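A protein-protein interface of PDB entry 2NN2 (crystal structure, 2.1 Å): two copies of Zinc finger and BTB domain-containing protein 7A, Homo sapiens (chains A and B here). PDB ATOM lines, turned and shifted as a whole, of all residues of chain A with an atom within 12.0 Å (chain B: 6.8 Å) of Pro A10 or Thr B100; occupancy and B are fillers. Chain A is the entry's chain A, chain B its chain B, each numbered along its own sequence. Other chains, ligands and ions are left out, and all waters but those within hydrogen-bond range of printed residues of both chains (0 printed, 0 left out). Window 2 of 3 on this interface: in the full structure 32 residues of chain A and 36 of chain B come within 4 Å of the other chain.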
ATOM      1  N   GLY A   9      30.954  34.616 -10.821  1.00  0.00           N
ATOM      2  CA  GLY A   9      30.721  33.743  -9.604  1.00  0.00           C
ATOM      3  C   GLY A   9      29.507  32.865  -9.855  1.00  0.00           C
ATOM      4  O   GLY A   9      28.858  33.009 -10.875  1.00  0.00           O
ATOM      5  N   PRO A  10      29.170  31.973  -8.916  1.00  0.00           N
ATOM      6  CA  PRO A  10      27.949  31.192  -9.126  1.00  0.00           C
ATOM      7  C   PRO A  10      26.671  32.027  -8.915  1.00  0.00           C
ATOM      8  O   PRO A  10      26.625  32.897  -8.059  1.00  0.00           O
ATOM      9  CB  PRO A  10      28.064  30.069  -8.110  1.00  0.00           C
ATOM     10  CG  PRO A  10      29.016  30.571  -7.045  1.00  0.00           C
ATOM     11  CD  PRO A  10      29.836  31.682  -7.636  1.00  0.00           C
ATOM     12  N   ILE A  11      25.668  31.769  -9.747  1.00  0.00           N
ATOM     13  CA  ILE A  11      24.340  32.339  -9.668  1.00  0.00           C
ATOM     14  C   ILE A  11      23.399  31.181  -9.282  1.00  0.00           C
ATOM     15  O   ILE A  11      23.423  30.121  -9.927  1.00  0.00           O
ATOM     16  CB  ILE A  11      23.937  32.828 -11.081  1.00  0.00           C
ATOM     17  CG1 ILE A  11      24.979  33.832 -11.628  1.00  0.00           C
ATOM     18  CG2 ILE A  11      22.562  33.362 -11.121  1.00  0.00           C
ATOM     19  CD1 ILE A  11      24.680  34.302 -13.040  1.00  0.00           C
ATOM     20  N   GLY A  12      22.583  31.370  -8.242  1.00  0.00           N
ATOM     21  CA  GLY A  12      21.516  30.435  -7.911  1.00  0.00           C
ATOM     22  C   GLY A  12      20.261  30.810  -8.661  1.00  0.00           C
ATOM     23  O   GLY A  12      19.862  31.974  -8.715  1.00  0.00           O
ATOM     24  N   ILE A  13      19.643  29.833  -9.298  1.00  0.00           N
ATOM     25  CA  ILE A  13      18.402  30.065 -10.020  1.00  0.00           C
ATOM     26  C   ILE A  13      17.309  29.166  -9.418  1.00  0.00           C
ATOM     27  O   ILE A  13      17.247  27.995  -9.757  1.00  0.00           O
ATOM     28  CB  ILE A  13      18.518  29.710 -11.512  1.00  0.00           C
ATOM     29  CG1 ILE A  13      19.744  30.388 -12.220  1.00  0.00           C
ATOM     30  CG2 ILE A  13      17.228  30.056 -12.199  1.00  0.00           C
ATOM     31  CD1 ILE A  13      20.017  29.743 -13.577  1.00  0.00           C
ATOM     32  N   PRO A  14      16.436  29.715  -8.538  1.00  0.00           N
ATOM     33  CA  PRO A  14      15.313  28.936  -7.914  1.00  0.00           C
ATOM     34  C   PRO A  14      14.119  28.714  -8.836  1.00  0.00           C
ATOM     35  O   PRO A  14      13.771  29.595  -9.635  1.00  0.00           O
ATOM     36  CB  PRO A  14      14.887  29.801  -6.715  1.00  0.00           C
ATOM     37  CG  PRO A  14      15.540  31.162  -6.897  1.00  0.00           C
ATOM     38  CD  PRO A  14      16.486  31.113  -8.086  1.00  0.00           C
ATOM     39  N   PHE A  15      13.494  27.546  -8.722  1.00  0.00           N
ATOM     40  CA  PHE A  15      12.366  27.125  -9.573  1.00  0.00           C
ATOM     41  C   PHE A  15      11.112  26.819  -8.678  1.00  0.00           C
ATOM     42  O   PHE A  15      10.966  25.678  -8.182  1.00  0.00           O
ATOM     43  CB  PHE A  15      12.767  25.880 -10.377  1.00  0.00           C
ATOM     44  CG  PHE A  15      13.714  26.178 -11.543  1.00  0.00           C
ATOM     45  CD1 PHE A  15      15.044  26.449 -11.335  1.00  0.00           C
ATOM     46  CD2 PHE A  15      13.245  26.227 -12.837  1.00  0.00           C
ATOM     47  CE1 PHE A  15      15.913  26.745 -12.426  1.00  0.00           C
ATOM     48  CE2 PHE A  15      14.113  26.532 -13.916  1.00  0.00           C
ATOM     49  CZ  PHE A  15      15.423  26.773 -13.690  1.00  0.00           C
ATOM     50  N   HIS A  18       8.965  23.631  -9.142  1.00  0.00           N
ATOM     51  CA  HIS A  18       9.680  22.380  -9.445  1.00  0.00           C
ATOM     52  C   HIS A  18       9.230  21.161  -8.600  1.00  0.00           C
ATOM     53  O   HIS A  18       8.981  20.097  -9.142  1.00  0.00           O
ATOM     54  CB  HIS A  18      11.184  22.561  -9.306  1.00  0.00           C
ATOM     55  CG  HIS A  18      11.942  21.317  -9.576  1.00  0.00           C
ATOM     56  ND1 HIS A  18      12.038  20.786 -10.835  1.00  0.00           N
ATOM     57  CD2 HIS A  18      12.605  20.470  -8.749  1.00  0.00           C
ATOM     58  CE1 HIS A  18      12.723  19.654 -10.779  1.00  0.00           C
ATOM     59  NE2 HIS A  18      13.060  19.429  -9.519  1.00  0.00           N
ATOM     60  N   ALA B  89      25.265  19.563 -11.791  1.00  0.00           N
ATOM     61  CA  ALA B  89      24.404  20.725 -11.621  1.00  0.00           C
ATOM     62  C   ALA B  89      22.946  20.355 -11.826  1.00  0.00           C
ATOM     63  O   ALA B  89      22.075  20.877 -11.106  1.00  0.00           O
ATOM     64  CB  ALA B  89      24.810  21.863 -12.612  1.00  0.00           C
ATOM     65  N   LEU B  90      22.687  19.474 -12.802  1.00  0.00           N
ATOM     66  CA  LEU B  90      21.321  19.160 -13.210  1.00  0.00           C
ATOM     67  C   LEU B  90      20.682  18.191 -12.185  1.00  0.00           C
ATOM     68  O   LEU B  90      19.503  18.287 -11.914  1.00  0.00           O
ATOM     69  CB  LEU B  90      21.282  18.578 -14.628  1.00  0.00           C
ATOM     70  CG  LEU B  90      21.495  19.587 -15.788  1.00  0.00           C
ATOM     71  CD1 LEU B  90      21.555  18.868 -17.128  1.00  0.00           C
ATOM     72  CD2 LEU B  90      20.397  20.657 -15.828  1.00  0.00           C
ATOM     73  N   ASP B  92      21.560  18.095  -8.822  1.00  0.00           N
ATOM     74  CA  ASP B  92      21.273  18.989  -7.733  1.00  0.00           C
ATOM     75  C   ASP B  92      19.956  19.754  -7.978  1.00  0.00           C
ATOM     76  O   ASP B  92      19.098  19.825  -7.072  1.00  0.00           O
ATOM     77  CB  ASP B  92      22.406  19.997  -7.532  1.00  0.00           C
ATOM     78  CG  ASP B  92      23.663  19.366  -6.932  1.00  0.00           C
ATOM     79  OD1 ASP B  92      23.654  18.118  -6.680  1.00  0.00           O
ATOM     80  OD2 ASP B  92      24.652  20.121  -6.727  1.00  0.00           O
ATOM     81  N   PHE B  93      19.801  20.343  -9.163  1.00  0.00           N
ATOM     82  CA  PHE B  93      18.504  20.918  -9.574  1.00  0.00           C
ATOM     83  C   PHE B  93      17.305  19.954  -9.363  1.00  0.00           C
ATOM     84  O   PHE B  93      16.331  20.340  -8.712  1.00  0.00           O
ATOM     85  CB  PHE B  93      18.530  21.421 -11.017  1.00  0.00           C
ATOM     86  CG  PHE B  93      17.170  21.647 -11.610  1.00  0.00           C
ATOM     87  CD1 PHE B  93      16.391  22.749 -11.226  1.00  0.00           C
ATOM     88  CD2 PHE B  93      16.649  20.750 -12.548  1.00  0.00           C
ATOM     89  CE1 PHE B  93      15.105  22.953 -11.790  1.00  0.00           C
ATOM     90  CE2 PHE B  93      15.382  20.947 -13.124  1.00  0.00           C
ATOM     91  CZ  PHE B  93      14.613  22.082 -12.759  1.00  0.00           C
ATOM     92  N   THR B  98      16.758  24.227  -7.078  1.00  0.00           N
ATOM     93  CA  THR B  98      17.637  25.364  -7.445  1.00  0.00           C
ATOM     94  C   THR B  98      18.735  24.887  -8.390  1.00  0.00           C
ATOM     95  O   THR B  98      19.339  23.867  -8.147  1.00  0.00           O
ATOM     96  CB  THR B  98      18.286  26.074  -6.175  1.00  0.00           C
ATOM     97  OG1 THR B  98      17.261  26.709  -5.434  1.00  0.00           O
ATOM     98  CG2 THR B  98      19.289  27.198  -6.542  1.00  0.00           C
ATOM     99  N   LEU B  99      18.960  25.626  -9.478  1.00  0.00           N
ATOM    100  CA  LEU B  99      20.030  25.349 -10.397  1.00  0.00           C
ATOM    101  C   LEU B  99      21.120  26.374 -10.141  1.00  0.00           C
ATOM    102  O   LEU B  99      20.845  27.604 -10.126  1.00  0.00           O
ATOM    103  CB  LEU B  99      19.554  25.432 -11.846  1.00  0.00           C
ATOM    104  CG  LEU B  99      20.651  25.277 -12.928  1.00  0.00           C
ATOM    105  CD1 LEU B  99      21.154  23.807 -13.041  1.00  0.00           C
ATOM    106  CD2 LEU B  99      20.153  25.798 -14.255  1.00  0.00           C
ATOM    107  N   THR B 100      22.327  25.883  -9.881  1.00  0.00           N
ATOM    108  CA  THR B 100      23.493  26.761  -9.694  1.00  0.00           C
ATOM    109  C   THR B 100      24.374  26.735 -10.975  1.00  0.00           C
ATOM    110  O   THR B 100      24.785  25.665 -11.418  1.00  0.00           O
ATOM    111  CB  THR B 100      24.308  26.373  -8.438  1.00  0.00           C
ATOM    112  OG1 THR B 100      23.438  26.224  -7.297  1.00  0.00           O
ATOM    113  CG2 THR B 100      25.323  27.421  -8.121  1.00  0.00           C
ATOM    114  N   VAL B 101      24.632  27.904 -11.566  1.00  0.00           N
ATOM    115  CA  VAL B 101      25.389  28.049 -12.807  1.00  0.00           C
ATOM    116  C   VAL B 101      26.432  29.142 -12.697  1.00  0.00           C
ATOM    117  O   VAL B 101      26.359  29.968 -11.804  1.00  0.00           O
ATOM    118  CB  VAL B 101      24.479  28.412 -14.046  1.00  0.00           C
ATOM    119  CG1 VAL B 101      23.351  27.491 -14.173  1.00  0.00           C
ATOM    120  CG2 VAL B 101      23.937  29.855 -13.922  1.00  0.00           C
ATOM    121  N   SER B 102      27.402  29.157 -13.611  1.00  0.00           N
ATOM    122  CA  SER B 102      28.288  30.331 -13.802  1.00  0.00           C
ATOM    123  C   SER B 102      28.413  30.761 -15.269  1.00  0.00           C
ATOM    124  O   SER B 102      28.009  30.025 -16.178  1.00  0.00           O
ATOM    125  CB  SER B 102      29.664  30.063 -13.253  1.00  0.00           C
ATOM    126  OG  SER B 102      30.398  29.259 -14.166  1.00  0.00           O
ATOM    127  N   THR B 103      28.961  31.965 -15.493  1.00  0.00           N
ATOM    128  CA  THR B 103      29.465  32.411 -16.810  1.00  0.00           C
ATOM    129  C   THR B 103      30.202  31.315 -17.586  1.00  0.00           C
ATOM    130  O   THR B 103      29.958  31.104 -18.781  1.00  0.00           O
ATOM    131  CB  THR B 103      30.477  33.593 -16.652  1.00  0.00           C
ATOM    132  OG1 THR B 103      31.391  33.320 -15.558  1.00  0.00           O
ATOM    133  CG2 THR B 103      29.754  34.862 -16.399  1.00  0.00           C
ATOM    134  N   ASN B 105      30.199  27.908 -17.173  1.00  0.00           N
ATOM    135  CA  ASN B 105      29.594  26.586 -17.428  1.00  0.00           C
ATOM    136  C   ASN B 105      28.154  26.601 -17.981  1.00  0.00           C
ATOM    137  O   ASN B 105      27.520  25.552 -18.124  1.00  0.00           O
ATOM    138  CB  ASN B 105      29.733  25.675 -16.206  1.00  0.00           C
ATOM    139  CG  ASN B 105      28.821  26.073 -15.057  1.00  0.00           C
ATOM    140  OD1 ASN B 105      27.940  26.916 -15.207  1.00  0.00           O
ATOM    141  ND2 ASN B 105      29.035  25.467 -13.900  1.00  0.00           N
ATOM    142  N   ILE B 109      25.699  23.492 -19.451  1.00  0.00           N
ATOM    143  CA  ILE B 109      24.432  23.127 -18.808  1.00  0.00           C
ATOM    144  C   ILE B 109      23.288  23.284 -19.796  1.00  0.00           C
ATOM    145  O   ILE B 109      22.378  22.462 -19.825  1.00  0.00           O
ATOM    146  CB  ILE B 109      24.189  23.955 -17.532  1.00  0.00           C
ATOM    147  CG1 ILE B 109      25.186  23.524 -16.437  1.00  0.00           C
ATOM    148  CG2 ILE B 109      22.746  23.774 -17.042  1.00  0.00           C
ATOM    149  CD1 ILE B 109      25.521  24.590 -15.404  1.00  0.00           C
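Of the 8 printed residues of chain A, 8 touch a printed residue of chain B. Hydrophobic or aromatic side chains of chain A within 4 Å of the printed part of chain B: Pro A10, Ile A11, Ile A13, Phe A15 and His A18. Along chain B the printed residues that touch a printed residue of chain A span positions 93 to 102. Among the printed residues, no Asp or Glu carboxylate lies within 4 Å of a Lys or Arg side-chain nitrogen of the other chain.
The backbone NH (N) of Ser B102 lies within hydrogen-bond range of the side-chain amide oxygen (OD1) of Asn B105 (2.8 Å).
No position is printed for both chains. Of the 14 pairs that touch across the chains among the printed residues, none has its exchanged pair printed and touching as well.
Pro A10 touches just these residues of chain B: Thr B100 and Val B101. Thr B100 touches just these residues of chain A: Pro A10 (3.8 Å) and Ile A11 (3.4 Å). No residue of chain A comes within 4 Å of Ala B89. Thr B98 touches just these residues of chain A: Ile A13 and Pro A14. Leu B99 touches just these residues of chain A: Ile A11, Gly A12, Ile A13 and Phe A15. Val B101 touches just these residues of chain A: Pro A10, Ile A11 and Ile A13. Printed residues of chain A within 4 Å of Ser B102: Gly A9 (3.9 Å). Printed residues of chain B within 4 Å of Pro A14: Thr B98. Of the printed residues of chain A, Phe B93 touches Phe A15 and His A18. Ile B109 touches none of the printed residues of chain A. The nearest residue of chain B that does not touch Pro A10 is Ser B102 (4.6 Å). The nearest residue of chain A that does not touch Thr B100 is Gly A12 (4.5 Å).
The backbone carbonyl oxygen (O) of Val B101 sits at hydrogen-bond distance from the backbone NH (N) of Ile A11. A ring nitrogen (NE2) of His A18 lies within hydrogen-bond range of the backbone carbonyl oxygen (O) of Phe B93. The backbone NH (N) of Ile A13 sits at hydrogen-bond distance from the backbone carbonyl oxygen (O) of Leu B99.
Among the printed residues, pairs that only touch across the chains: Gly A9 with Ser B102 (3.9 Å), Pro A10 with Thr B100 (3.8 Å), Pro A10 with Val B101 (3.3 Å), Ile A11 with Leu B99 (3.6 Å), Ile A11 with Thr B100 (3.4 Å), Gly A12 with Leu B99 (3.6 Å), Ile A13 with Thr B98 (3.5 Å), Ile A13 with Val B101 (3.9 Å), Pro A14 with Thr B98 (3.9 Å), Phe A15 with Phe B93 (3.5 Å) and Phe A15 with Leu B99 (3.9 Å).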
